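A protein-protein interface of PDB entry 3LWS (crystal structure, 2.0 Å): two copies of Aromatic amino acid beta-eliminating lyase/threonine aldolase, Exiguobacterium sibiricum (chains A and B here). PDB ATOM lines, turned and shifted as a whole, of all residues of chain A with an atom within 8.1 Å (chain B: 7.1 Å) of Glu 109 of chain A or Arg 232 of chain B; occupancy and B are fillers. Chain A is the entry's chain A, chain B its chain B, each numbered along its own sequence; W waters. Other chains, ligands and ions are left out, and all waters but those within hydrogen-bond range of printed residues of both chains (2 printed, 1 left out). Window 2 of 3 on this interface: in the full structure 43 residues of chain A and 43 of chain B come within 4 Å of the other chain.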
ATOM      1  N   SER A  70     -23.823   1.659  -4.482  1.00  0.00           N
ATOM      2  CA  SER A  70     -22.591   1.110  -3.904  1.00  0.00           C
ATOM      3  C   SER A  70     -22.737   0.591  -2.479  1.00  0.00           C
ATOM      4  O   SER A  70     -23.571   1.041  -1.700  1.00  0.00           O
ATOM      5  CB  SER A  70     -21.512   2.185  -3.941  1.00  0.00           C
ATOM      6  OG  SER A  70     -21.835   3.281  -3.093  1.00  0.00           O
ATOM      7  N   THR A  72     -20.298   1.151  -0.514  1.00  0.00           N
ATOM      8  CA  THR A  72     -19.676   2.231   0.238  1.00  0.00           C
ATOM      9  C   THR A  72     -20.754   3.097   0.856  1.00  0.00           C
ATOM     10  O   THR A  72     -20.753   3.310   2.073  1.00  0.00           O
ATOM     11  CB  THR A  72     -18.674   3.031  -0.632  1.00  0.00           C
ATOM     12  OG1 THR A  72     -17.519   2.205  -0.823  1.00  0.00           O
ATOM     13  CG2 THR A  72     -18.260   4.365   0.052  1.00  0.00           C
ATOM     14  N   MET A  73     -21.696   3.536   0.019  1.00  0.00           N
ATOM     15  CA  MET A  73     -22.860   4.311   0.450  1.00  0.00           C
ATOM     16  C   MET A  73     -23.749   3.500   1.376  1.00  0.00           C
ATOM     17  O   MET A  73     -24.128   3.961   2.450  1.00  0.00           O
ATOM     18  CB  MET A  73     -23.674   4.764  -0.758  1.00  0.00           C
ATOM     19  CG  MET A  73     -24.776   5.736  -0.422  1.00  0.00           C
ATOM     20  SD  MET A  73     -25.895   6.191  -1.935  1.00  0.00           S
ATOM     21  CE  MET A  73     -24.577   7.065  -3.183  1.00  0.00           C
ATOM     22  N   GLN A  76     -22.167   2.946   5.121  1.00  0.00           N
ATOM     23  CA  GLN A  76     -22.167   4.231   5.805  1.00  0.00           C
ATOM     24  C   GLN A  76     -23.559   4.568   6.275  1.00  0.00           C
ATOM     25  O   GLN A  76     -23.766   4.915   7.454  1.00  0.00           O
ATOM     26  CB  GLN A  76     -21.653   5.344   4.906  1.00  0.00           C
ATOM     27  CG  GLN A  76     -20.145   5.389   4.843  1.00  0.00           C
ATOM     28  CD  GLN A  76     -19.631   6.379   3.837  1.00  0.00           C
ATOM     29  OE1 GLN A  76     -20.223   7.437   3.639  1.00  0.00           O
ATOM     30  NE2 GLN A  76     -18.504   6.061   3.209  1.00  0.00           N
ATOM     31  N   HIS A 102     -10.753   1.965   2.566  1.00  0.00           N
ATOM     32  CA  HIS A 102     -10.965   2.045   1.118  1.00  0.00           C
ATOM     33  C   HIS A 102     -12.017   3.109   0.701  1.00  0.00           C
ATOM     34  O   HIS A 102     -12.413   3.140  -0.449  1.00  0.00           O
ATOM     35  CB  HIS A 102     -11.354   0.667   0.580  1.00  0.00           C
ATOM     36  CG  HIS A 102     -10.247  -0.334   0.570  1.00  0.00           C
ATOM     37  ND1 HIS A 102      -9.087  -0.146  -0.146  1.00  0.00           N
ATOM     38  CD2 HIS A 102     -10.139  -1.553   1.149  1.00  0.00           C
ATOM     39  CE1 HIS A 102      -8.305  -1.200   0.000  1.00  0.00           C
ATOM     40  NE2 HIS A 102      -8.914  -2.067   0.784  1.00  0.00           N
ATOM     41  N   GLU A 103     -12.451   3.991   1.602  1.00  0.00           N
ATOM     42  CA  GLU A 103     -13.559   4.932   1.270  1.00  0.00           C
ATOM     43  C   GLU A 103     -13.203   6.421   1.477  1.00  0.00           C
ATOM     44  O   GLU A 103     -14.080   7.304   1.548  1.00  0.00           O
ATOM     45  CB  GLU A 103     -14.826   4.531   2.031  1.00  0.00           C
ATOM     46  CG  GLU A 103     -15.368   3.153   1.646  1.00  0.00           C
ATOM     47  CD  GLU A 103     -16.529   2.687   2.499  1.00  0.00           C
ATOM     48  OE1 GLU A 103     -17.181   3.524   3.148  1.00  0.00           O
ATOM     49  OE2 GLU A 103     -16.753   1.472   2.549  1.00  0.00           O
ATOM     50  N   GLN A 104     -11.902   6.693   1.475  1.00  0.00           N
ATOM     51  CA  GLN A 104     -11.367   8.028   1.720  1.00  0.00           C
ATOM     52  C   GLN A 104     -12.010   8.620   3.029  1.00  0.00           C
ATOM     53  O   GLN A 104     -12.362   9.790   3.105  1.00  0.00           O
ATOM     54  CB  GLN A 104     -11.561   8.932   0.480  1.00  0.00           C
ATOM     55  CG  GLN A 104     -10.630   8.668  -0.698  1.00  0.00           C
ATOM     56  CD  GLN A 104      -9.201   9.084  -0.413  1.00  0.00           C
ATOM     57  OE1 GLN A 104      -8.940   9.783   0.545  1.00  0.00           O
ATOM     58  NE2 GLN A 104      -8.270   8.605  -1.210  1.00  0.00           N
ATOM     59  N   ASP A 105     -12.141   7.766   4.045  1.00  0.00           N
ATOM     60  CA  ASP A 105     -12.628   8.121   5.363  1.00  0.00           C
ATOM     61  C   ASP A 105     -14.054   8.628   5.365  1.00  0.00           C
ATOM     62  O   ASP A 105     -14.438   9.399   6.267  1.00  0.00           O
ATOM     63  CB  ASP A 105     -11.727   9.185   5.972  1.00  0.00           C
ATOM     64  CG  ASP A 105     -10.279   8.764   5.986  1.00  0.00           C
ATOM     65  OD1 ASP A 105      -9.994   7.702   6.579  1.00  0.00           O
ATOM     66  OD2 ASP A 105      -9.448   9.504   5.406  1.00  0.00           O
ATOM     67  N   GLY A 106     -14.829   8.181   4.366  1.00  0.00           N
ATOM     68  CA  GLY A 106     -16.187   8.663   4.111  1.00  0.00           C
ATOM     69  C   GLY A 106     -17.059   8.663   5.336  1.00  0.00           C
ATOM     70  O   GLY A 106     -17.672   9.676   5.636  1.00  0.00           O
ATOM     71  N   LEU A 107     -17.081   7.542   6.070  1.00  0.00           N
ATOM     72  CA  LEU A 107     -17.891   7.433   7.295  1.00  0.00           C
ATOM     73  C   LEU A 107     -17.634   8.609   8.275  1.00  0.00           C
ATOM     74  O   LEU A 107     -18.564   9.267   8.756  1.00  0.00           O
ATOM     75  CB  LEU A 107     -17.579   6.107   8.016  1.00  0.00           C
ATOM     76  CG  LEU A 107     -18.367   5.783   9.294  1.00  0.00           C
ATOM     77  CD1 LEU A 107     -19.897   5.880   9.033  1.00  0.00           C
ATOM     78  CD2 LEU A 107     -17.968   4.393   9.801  1.00  0.00           C
ATOM     79  N   LYS A 108     -16.364   8.887   8.526  1.00  0.00           N
ATOM     80  CA  LYS A 108     -15.981   9.877   9.506  1.00  0.00           C
ATOM     81  C   LYS A 108     -16.076  11.292   8.967  1.00  0.00           C
ATOM     82  O   LYS A 108     -16.215  12.215   9.742  1.00  0.00           O
ATOM     83  CB  LYS A 108     -14.559   9.615  10.010  1.00  0.00           C
ATOM     84  CG  LYS A 108     -14.343   8.240  10.664  1.00  0.00           C
ATOM     85  CD  LYS A 108     -12.853   7.961  10.902  1.00  0.00           C
ATOM     86  CE  LYS A 108     -12.543   6.473  11.083  1.00  0.00           C
ATOM     87  NZ  LYS A 108     -11.058   6.148  11.077  1.00  0.00           N
ATOM     88  N   GLU A 109     -15.994  11.473   7.656  1.00  0.00           N
ATOM     89  CA  GLU A 109     -16.053  12.811   7.083  1.00  0.00           C
ATOM     90  C   GLU A 109     -17.495  13.201   6.942  1.00  0.00           C
ATOM     91  O   GLU A 109     -17.798  14.361   7.051  1.00  0.00           O
ATOM     92  CB  GLU A 109     -15.364  12.857   5.714  1.00  0.00           C
ATOM     93  CG  GLU A 109     -13.848  12.660   5.780  1.00  0.00           C
ATOM     94  CD  GLU A 109     -13.059  13.917   6.219  1.00  0.00           C
ATOM     95  OE1 GLU A 109     -13.541  15.055   6.064  1.00  0.00           O
ATOM     96  OE2 GLU A 109     -11.934  13.759   6.722  1.00  0.00           O
ATOM     97  N   LEU A 110     -18.386  12.222   6.724  1.00  0.00           N
ATOM     98  CA  LEU A 110     -19.797  12.497   6.438  1.00  0.00           C
ATOM     99  C   LEU A 110     -20.759  12.360   7.623  1.00  0.00           C
ATOM    100  O   LEU A 110     -21.899  12.822   7.547  1.00  0.00           O
ATOM    101  CB  LEU A 110     -20.258  11.622   5.260  1.00  0.00           C
ATOM    102  CG  LEU A 110     -19.682  12.055   3.904  1.00  0.00           C
ATOM    103  CD1 LEU A 110     -20.013  11.005   2.915  1.00  0.00           C
ATOM    104  CD2 LEU A 110     -20.214  13.469   3.471  1.00  0.00           C
ATOM    105  N   HIS A 111     -20.296  11.756   8.712  1.00  0.00           N
ATOM    106  CA  HIS A 111     -21.095  11.572   9.912  1.00  0.00           C
ATOM    107  C   HIS A 111     -20.222  11.762  11.155  1.00  0.00           C
ATOM    108  O   HIS A 111     -19.018  11.481  11.122  1.00  0.00           O
ATOM    109  CB  HIS A 111     -21.712  10.166   9.922  1.00  0.00           C
ATOM    110  CG  HIS A 111     -22.390   9.817   8.644  1.00  0.00           C
ATOM    111  ND1 HIS A 111     -23.711  10.126   8.394  1.00  0.00           N
ATOM    112  CD2 HIS A 111     -21.911   9.243   7.519  1.00  0.00           C
ATOM    113  CE1 HIS A 111     -24.020   9.740   7.175  1.00  0.00           C
ATOM    114  NE2 HIS A 111     -22.942   9.211   6.618  1.00  0.00           N
ATOM    115  N   PRO A 112     -20.817  12.256  12.265  1.00  0.00           N
ATOM    116  CA  PRO A 112     -20.017  12.450  13.469  1.00  0.00           C
ATOM    117  C   PRO A 112     -19.856  11.092  14.155  1.00  0.00           C
ATOM    118  O   PRO A 112     -20.426  10.851  15.206  1.00  0.00           O
ATOM    119  CB  PRO A 112     -20.860  13.452  14.284  1.00  0.00           C
ATOM    120  CG  PRO A 112     -22.241  13.209  13.878  1.00  0.00           C
ATOM    121  CD  PRO A 112     -22.172  12.806  12.415  1.00  0.00           C
ATOM    122  N   ILE A 113     -19.105  10.196  13.518  1.00  0.00           N
ATOM    123  CA  ILE A 113     -18.980   8.837  13.992  1.00  0.00           C
ATOM    124  C   ILE A 113     -17.500   8.430  14.163  1.00  0.00           C
ATOM    125  O   ILE A 113     -16.617   8.768  13.337  1.00  0.00           O
ATOM    126  CB  ILE A 113     -19.776   7.838  13.116  1.00  0.00           C
ATOM    127  CG1 ILE A 113     -21.286   8.111  13.208  1.00  0.00           C
ATOM    128  CG2 ILE A 113     -19.469   6.401  13.546  1.00  0.00           C
ATOM    129  CD1 ILE A 113     -22.136   7.301  12.291  1.00  0.00           C
ATOM    130  N   TYR A 233     -27.716  11.287  -0.076  1.00  0.00           N
ATOM    131  CA  TYR A 233     -26.422  10.973  -0.713  1.00  0.00           C
ATOM    132  C   TYR A 233     -26.361  11.177  -2.225  1.00  0.00           C
ATOM    133  O   TYR A 233     -25.303  11.117  -2.801  1.00  0.00           O
ATOM    134  CB  TYR A 233     -26.069   9.508  -0.429  1.00  0.00           C
ATOM    135  CG  TYR A 233     -25.190   9.241   0.781  1.00  0.00           C
ATOM    136  CD1 TYR A 233     -25.727   9.129   2.058  1.00  0.00           C
ATOM    137  CD2 TYR A 233     -23.814   9.020   0.632  1.00  0.00           C
ATOM    138  CE1 TYR A 233     -24.912   8.839   3.171  1.00  0.00           C
ATOM    139  CE2 TYR A 233     -23.007   8.731   1.742  1.00  0.00           C
ATOM    140  CZ  TYR A 233     -23.579   8.638   2.995  1.00  0.00           C
ATOM    141  OH  TYR A 233     -22.797   8.369   4.105  1.00  0.00           O
ATOM    142  N   ARG B  80     -19.446  22.217  -0.884  1.00  0.00           N
ATOM    143  CA  ARG B  80     -18.527  21.935   0.235  1.00  0.00           C
ATOM    144  C   ARG B  80     -17.093  22.292  -0.070  1.00  0.00           C
ATOM    145  O   ARG B  80     -16.397  22.826   0.800  1.00  0.00           O
ATOM    146  CB  ARG B  80     -18.630  20.479   0.694  1.00  0.00           C
ATOM    147  CG  ARG B  80     -17.646  20.065   1.811  1.00  0.00           C
ATOM    148  CD  ARG B  80     -17.986  20.708   3.155  1.00  0.00           C
ATOM    149  NE  ARG B  80     -17.018  20.259   4.158  1.00  0.00           N
ATOM    150  CZ  ARG B  80     -17.129  19.180   4.931  1.00  0.00           C
ATOM    151  NH1 ARG B  80     -18.193  18.384   4.882  1.00  0.00           N
ATOM    152  NH2 ARG B  80     -16.158  18.880   5.789  1.00  0.00           N
ATOM    153  N   ASP B  84     -15.098  24.926   2.120  1.00  0.00           N
ATOM    154  CA  ASP B  84     -13.716  24.673   2.554  1.00  0.00           C
ATOM    155  C   ASP B  84     -12.646  25.625   2.007  1.00  0.00           C
ATOM    156  O   ASP B  84     -11.793  26.118   2.757  1.00  0.00           O
ATOM    157  CB  ASP B  84     -13.302  23.245   2.181  1.00  0.00           C
ATOM    158  CG  ASP B  84     -13.987  22.211   3.005  1.00  0.00           C
ATOM    159  OD1 ASP B  84     -14.596  22.566   4.052  1.00  0.00           O
ATOM    160  OD2 ASP B  84     -13.883  21.041   2.601  1.00  0.00           O
ATOM    161  N   LEU B 110     -25.459  16.311   5.615  1.00  0.00           N
ATOM    162  CA  LEU B 110     -24.139  15.733   5.415  1.00  0.00           C
ATOM    163  C   LEU B 110     -22.943  16.694   5.597  1.00  0.00           C
ATOM    164  O   LEU B 110     -21.767  16.267   5.578  1.00  0.00           O
ATOM    165  CB  LEU B 110     -24.084  15.103   4.037  1.00  0.00           C
ATOM    166  CG  LEU B 110     -25.026  13.937   3.853  1.00  0.00           C
ATOM    167  CD1 LEU B 110     -25.073  13.596   2.379  1.00  0.00           C
ATOM    168  CD2 LEU B 110     -24.560  12.758   4.668  1.00  0.00           C
ATOM    169  N   HIS B 111     -23.220  17.980   5.748  1.00  0.00           N
ATOM    170  CA  HIS B 111     -22.161  18.983   5.816  1.00  0.00           C
ATOM    171  C   HIS B 111     -22.566  20.071   6.828  1.00  0.00           C
ATOM    172  O   HIS B 111     -23.751  20.379   6.930  1.00  0.00           O
ATOM    173  CB  HIS B 111     -21.934  19.630   4.446  1.00  0.00           C
ATOM    174  CG  HIS B 111     -21.658  18.654   3.344  1.00  0.00           C
ATOM    175  ND1 HIS B 111     -20.449  18.006   3.212  1.00  0.00           N
ATOM    176  CD2 HIS B 111     -22.437  18.201   2.333  1.00  0.00           C
ATOM    177  CE1 HIS B 111     -20.479  17.224   2.147  1.00  0.00           C
ATOM    178  NE2 HIS B 111     -21.681  17.315   1.600  1.00  0.00           N
ATOM    179  N   PRO B 112     -21.586  20.704   7.505  1.00  0.00           N
ATOM    180  CA  PRO B 112     -21.858  21.753   8.498  1.00  0.00           C
ATOM    181  C   PRO B 112     -22.097  23.077   7.781  1.00  0.00           C
ATOM    182  O   PRO B 112     -21.379  24.083   7.987  1.00  0.00           O
ATOM    183  CB  PRO B 112     -20.564  21.783   9.300  1.00  0.00           C
ATOM    184  CG  PRO B 112     -19.509  21.492   8.271  1.00  0.00           C
ATOM    185  CD  PRO B 112     -20.136  20.533   7.310  1.00  0.00           C
ATOM    186  N   THR B 225     -10.194  17.357  -5.680  1.00  0.00           N
ATOM    187  CA  THR B 225     -10.937  17.246  -4.429  1.00  0.00           C
ATOM    188  C   THR B 225     -12.339  16.702  -4.615  1.00  0.00           C
ATOM    189  O   THR B 225     -12.872  15.967  -3.750  1.00  0.00           O
ATOM    190  CB  THR B 225     -11.081  18.602  -3.756  1.00  0.00           C
ATOM    191  OG1 THR B 225      -9.775  19.086  -3.494  1.00  0.00           O
ATOM    192  CG2 THR B 225     -11.821  18.459  -2.461  1.00  0.00           C
ATOM    193  N   ALA B 226     -12.964  17.082  -5.707  1.00  0.00           N
ATOM    194  CA  ALA B 226     -14.298  16.529  -5.998  1.00  0.00           C
ATOM    195  C   ALA B 226     -14.227  15.024  -6.240  1.00  0.00           C
ATOM    196  O   ALA B 226     -15.148  14.325  -5.873  1.00  0.00           O
ATOM    197  CB  ALA B 226     -14.962  17.255  -7.155  1.00  0.00           C
ATOM    198  N   ARG B 227     -13.160  14.513  -6.841  1.00  0.00           N
ATOM    199  CA  ARG B 227     -13.008  13.068  -6.942  1.00  0.00           C
ATOM    200  C   ARG B 227     -12.819  12.374  -5.584  1.00  0.00           C
ATOM    201  O   ARG B 227     -13.212  11.234  -5.426  1.00  0.00           O
ATOM    202  CB  ARG B 227     -11.901  12.669  -7.900  1.00  0.00           C
ATOM    203  CG  ARG B 227     -12.239  12.935  -9.327  1.00  0.00           C
ATOM    204  CD  ARG B 227     -11.161  12.411 -10.275  1.00  0.00           C
ATOM    205  NE  ARG B 227     -11.475  12.819 -11.643  1.00  0.00           N
ATOM    206  CZ  ARG B 227     -11.036  13.930 -12.245  1.00  0.00           C
ATOM    207  NH1 ARG B 227     -10.187  14.761 -11.646  1.00  0.00           N
ATOM    208  NH2 ARG B 227     -11.436  14.203 -13.474  1.00  0.00           N
ATOM    209  N   ILE B 228     -12.251  13.052  -4.588  1.00  0.00           N
ATOM    210  CA  ILE B 228     -12.143  12.451  -3.270  1.00  0.00           C
ATOM    211  C   ILE B 228     -13.519  12.329  -2.622  1.00  0.00           C
ATOM    212  O   ILE B 228     -13.858  11.268  -2.077  1.00  0.00           O
ATOM    213  CB  ILE B 228     -11.125  13.193  -2.365  1.00  0.00           C
ATOM    214  CG1 ILE B 228      -9.727  13.062  -2.938  1.00  0.00           C
ATOM    215  CG2 ILE B 228     -11.191  12.659  -0.918  1.00  0.00           C
ATOM    216  CD1 ILE B 228      -8.837  14.257  -2.673  1.00  0.00           C
ATOM    217  N   TRP B 229     -14.326  13.387  -2.715  1.00  0.00           N
ATOM    218  CA  TRP B 229     -15.657  13.372  -2.135  1.00  0.00           C
ATOM    219  C   TRP B 229     -16.540  12.372  -2.828  1.00  0.00           C
ATOM    220  O   TRP B 229     -17.337  11.730  -2.145  1.00  0.00           O
ATOM    221  CB  TRP B 229     -16.340  14.742  -2.139  1.00  0.00           C
ATOM    222  CG  TRP B 229     -15.846  15.734  -1.093  1.00  0.00           C
ATOM    223  CD1 TRP B 229     -15.076  16.804  -1.317  1.00  0.00           C
ATOM    224  CD2 TRP B 229     -16.124  15.729   0.330  1.00  0.00           C
ATOM    225  NE1 TRP B 229     -14.856  17.493  -0.135  1.00  0.00           N
ATOM    226  CE2 TRP B 229     -15.473  16.839   0.886  1.00  0.00           C
ATOM    227  CE3 TRP B 229     -16.843  14.897   1.165  1.00  0.00           C
ATOM    228  CZ2 TRP B 229     -15.534  17.138   2.232  1.00  0.00           C
ATOM    229  CZ3 TRP B 229     -16.926  15.200   2.484  1.00  0.00           C
ATOM    230  CH2 TRP B 229     -16.263  16.311   3.018  1.00  0.00           C
ATOM    231  N   LYS B 230     -16.401  12.221  -4.155  1.00  0.00           N
ATOM    232  CA  LYS B 230     -17.125  11.172  -4.904  1.00  0.00           C
ATOM    233  C   LYS B 230     -16.927   9.767  -4.316  1.00  0.00           C
ATOM    234  O   LYS B 230     -17.893   8.998  -4.219  1.00  0.00           O
ATOM    235  CB  LYS B 230     -16.810  11.179  -6.409  1.00  0.00           C
ATOM    236  CG  LYS B 230     -17.616  10.100  -7.182  1.00  0.00           C
ATOM    237  CD  LYS B 230     -17.501  10.229  -8.700  1.00  0.00           C
ATOM    238  CE  LYS B 230     -16.090  10.031  -9.186  1.00  0.00           C
ATOM    239  NZ  LYS B 230     -16.063   9.857 -10.693  1.00  0.00           N
ATOM    240  N   ARG B 231     -15.695   9.457  -3.901  1.00  0.00           N
ATOM    241  CA  ARG B 231     -15.435   8.178  -3.241  1.00  0.00           C
ATOM    242  C   ARG B 231     -16.049   8.149  -1.839  1.00  0.00           C
ATOM    243  O   ARG B 231     -16.711   7.168  -1.481  1.00  0.00           O
ATOM    244  CB  ARG B 231     -13.939   7.818  -3.233  1.00  0.00           C
ATOM    245  CG  ARG B 231     -13.601   6.590  -2.381  1.00  0.00           C
ATOM    246  CD  ARG B 231     -12.620   5.650  -3.066  1.00  0.00           C
ATOM    247  NE  ARG B 231     -13.285   4.868  -4.101  1.00  0.00           N
ATOM    248  CZ  ARG B 231     -14.193   3.927  -3.855  1.00  0.00           C
ATOM    249  NH1 ARG B 231     -14.754   3.273  -4.864  1.00  0.00           N
ATOM    250  NH2 ARG B 231     -14.548   3.645  -2.602  1.00  0.00           N
ATOM    251  N   ARG B 232     -15.880   9.224  -1.060  1.00  0.00           N
ATOM    252  CA  ARG B 232     -16.484   9.301   0.271  1.00  0.00           C
ATOM    253  C   ARG B 232     -17.966   9.015   0.197  1.00  0.00           C
ATOM    254  O   ARG B 232     -18.466   8.206   0.972  1.00  0.00           O
ATOM    255  CB  ARG B 232     -16.203  10.679   0.921  1.00  0.00           C
ATOM    256  CG  ARG B 232     -14.783  10.860   1.284  1.00  0.00           C
ATOM    257  CD  ARG B 232     -14.506  12.235   1.793  1.00  0.00           C
ATOM    258  NE  ARG B 232     -13.081  12.425   2.019  1.00  0.00           N
ATOM    259  CZ  ARG B 232     -12.519  13.590   2.330  1.00  0.00           C
ATOM    260  NH1 ARG B 232     -13.254  14.685   2.501  1.00  0.00           N
ATOM    261  NH2 ARG B 232     -11.218  13.662   2.495  1.00  0.00           N
ATOM    262  N   TYR B 233     -18.644   9.649  -0.776  1.00  0.00           N
ATOM    263  CA  TYR B 233     -20.078   9.492  -1.019  1.00  0.00           C
ATOM    264  C   TYR B 233     -20.553   8.127  -1.478  1.00  0.00           C
ATOM    265  O   TYR B 233     -21.731   7.885  -1.474  1.00  0.00           O
ATOM    266  CB  TYR B 233     -20.572  10.507  -2.088  1.00  0.00           C
ATOM    267  CG  TYR B 233     -21.126  11.801  -1.520  1.00  0.00           C
ATOM    268  CD1 TYR B 233     -20.269  12.832  -1.137  1.00  0.00           C
ATOM    269  CD2 TYR B 233     -22.502  11.982  -1.351  1.00  0.00           C
ATOM    270  CE1 TYR B 233     -20.773  14.006  -0.599  1.00  0.00           C
ATOM    271  CE2 TYR B 233     -23.021  13.170  -0.857  1.00  0.00           C
ATOM    272  CZ  TYR B 233     -22.139  14.185  -0.475  1.00  0.00           C
ATOM    273  OH  TYR B 233     -22.615  15.367   0.063  1.00  0.00           O
ATOM    274  N   GLY B 234     -19.651   7.243  -1.898  1.00  0.00           N
ATOM    275  CA  GLY B 234     -20.069   6.001  -2.522  1.00  0.00           C
ATOM    276  C   GLY B 234     -20.561   6.201  -3.960  1.00  0.00           C
ATOM    277  O   GLY B 234     -21.361   5.427  -4.457  1.00  0.00           O
ATOM    278  N   GLY B 235     -20.044   7.218  -4.625  1.00  0.00           N
ATOM    279  CA  GLY B 235     -20.415   7.522  -6.006  1.00  0.00           C
ATOM    280  C   GLY B 235     -19.364   7.097  -7.002  1.00  0.00           C
ATOM    281  O   GLY B 235     -19.594   7.202  -8.210  1.00  0.00           O
ATOM    282  N   ASP B 236     -18.224   6.614  -6.497  1.00  0.00           N
ATOM    283  CA  ASP B 236     -17.039   6.249  -7.317  1.00  0.00           C
ATOM    284  C   ASP B 236     -17.118   4.763  -7.558  1.00  0.00           C
ATOM    285  O   ASP B 236     -16.361   3.964  -7.003  1.00  0.00           O
ATOM    286  CB  ASP B 236     -15.701   6.626  -6.635  1.00  0.00           C
ATOM    287  CG  ASP B 236     -14.485   6.218  -7.452  1.00  0.00           C
ATOM    288  OD1 ASP B 236     -14.577   6.206  -8.698  1.00  0.00           O
ATOM    289  OD2 ASP B 236     -13.433   5.926  -6.836  1.00  0.00           O
HETATM  290  O   HOH W   1     -15.951  16.430   7.282  1.00  0.00           O
HETATM  291  O   HOH W   2     -19.350  16.664   6.730  1.00  0.00           O
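The side-chain hydroxyl of Ser 70 of chain A is in hydrogen-bond range of the backbone carbonyl oxygen of Gly 234 of chain B.
The side-chain amide nitrogen of Gln 76 of chain A lies within hydrogen-bond range of the backbone carbonyl oxygen of Arg 232 of chain B (3.1 Å).
The guanidinium group (NH2) of Arg 231 of chain B is in hydrogen-bond range of the backbone carbonyl oxygen (O) of His 102 of chain A.
The backbone carbonyl oxygen (O) of Gln 104 of chain A is in hydrogen-bond range of the guanidinium group (NE) of Arg 232 of chain B (2.9 Å).
NH1 of Arg 232 of chain B lies within salt-bridge range of OE1 of Glu 109 of chain A (3.6 Å).
Of the 17 printed residues of chain A, 12 touch a printed residue of chain B.
Hydrophobic or aromatic side chains of chain A that line the printed part of chain B: Met 73, Leu 110, His 111 and Tyr 233.
Hydrophobic or aromatic side chains of chain B that line the printed part of chain A: Leu 110, His 111, Ile 228, Trp 229 and Tyr 233.
Among the printed residues, Asp or Glu carboxylates within 4 Å of a Lys or Arg side-chain nitrogen of the other chain: Glu 109 of chain A with Arg 232 of chain B.
Leu 110 of chain B touches its own counterpart, Leu 110 of chain A.
Leu 110 of chain A touches His 111 of chain B, and with the chains exchanged His 111 of chain A touches Leu 110 of chain B.
Tyr 233 of chain A touches its own counterpart, Tyr 233 of chain B.
Of the 21 pairs that touch across the chains among the printed residues, 4 have their exchanged pair printed and touching as well.
Among the printed residues, merely in contact across the chains: Thr 72 of chain A with Arg 231 of chain B (3.6 Å), Thr 72 of chain A with Arg 232 of chain B (3.96 Å), Thr 72 of chain A with Gly 234 of chain B (3.5 Å), Met 73 of chain A with Tyr 233 of chain B (3.4 Å), Met 73 of chain A with Gly 234 of chain B (3.8 Å), Glu 103 of chain A with Arg 231 of chain B (3.9 Å), Glu 103 of chain A with Arg 232 of chain B (3.4 Å), Gln 104 of chain A with Ile 228 of chain B (3.9 Å), Gln 104 of chain A with Arg 231 of chain B (3.997 Å), Gly 106 of chain A with Arg 232 of chain B (3.8 Å), Leu 110 of chain A with Leu 110 of chain B (3.8 Å), Leu 110 of chain A with His 111 of chain B (3.99 Å), Leu 110 of chain A with Trp 229 of chain B (3.8 Å), Leu 110 of chain A with Arg 232 of chain B (3.7 Å), His 111 of chain A with Leu 110 of chain B (3.96 Å) and Tyr 233 of chain A with Tyr 233 of chain B (3.2 Å).
The side-chain carboxylate (OE1) of Glu 103 of chain A is in hydrogen-bond range of the side-chain amide nitrogen (NE2) of Gln 76 of chain A.
OH of Tyr 233 of chain A lies within hydrogen-bond range of OE1 of Gln 76 of chain A (2.8 Å).
The side-chain hydroxyl (OH) of Tyr 233 of chain A sits at hydrogen-bond distance from a ring nitrogen (NE2) of His 111 of chain A (2.7 Å).
ND1 of His 111 of chain B sits at hydrogen-bond distance from NH1 of Arg 80 of chain B, at 2.8 Å.
The side-chain hydroxyl (OH) of Tyr 233 of chain B sits at hydrogen-bond distance from a ring nitrogen (NE2) of His 111 of chain B.
The side-chain carboxylate (OD2) of Asp 236 of chain B is in salt-bridge range of the guanidinium group (NE) of Arg 231 of chain B.
Water W2 lies within hydrogen-bond range of the backbone carbonyl oxygen of Leu 110 of chain B (2.7 Å), the guanidinium group of Arg 80 of chain B (2.8 Å) and the backbone carbonyl oxygen of Glu 109 of chain A (2.8 Å).
Water W1 lies within hydrogen-bond range of the backbone carbonyl oxygen of Glu 109 of chain A (2.8 Å) and the guanidinium group of Arg 80 of chain B (2.9 Å).
Of chain B, only Arg 232 comes within 4 Å of Glu 109 of chain A.
Arg 232 of chain B touches just these residues of chain A: Thr 72 (3.96 Å), Gln 76 (3.1 Å), Glu 103 (3.4 Å), Gln 104 (2.9 Å), Gly 106 (3.8 Å), Glu 109 (3.6 Å) and Leu 110 (3.7 Å).
Of the printed residues of chain B, Leu 110 of chain A touches Leu 110, His 111, Trp 229 and Arg 232.
Printed residues of chain B within 4 Å of Met 73 of chain A: Tyr 233 (3.4 Å) and Gly 234 (3.8 Å).
Of the printed residues of chain B, Glu 103 of chain A touches Arg 231 (3.9 Å) and Arg 232 (3.4 Å).
Lys 230 of chain B touches none of the printed residues of chain A.
The nearest printed residue of chain A that does not touch Tyr 233 of chain B is Leu 110 of chain A (4.1 Å).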
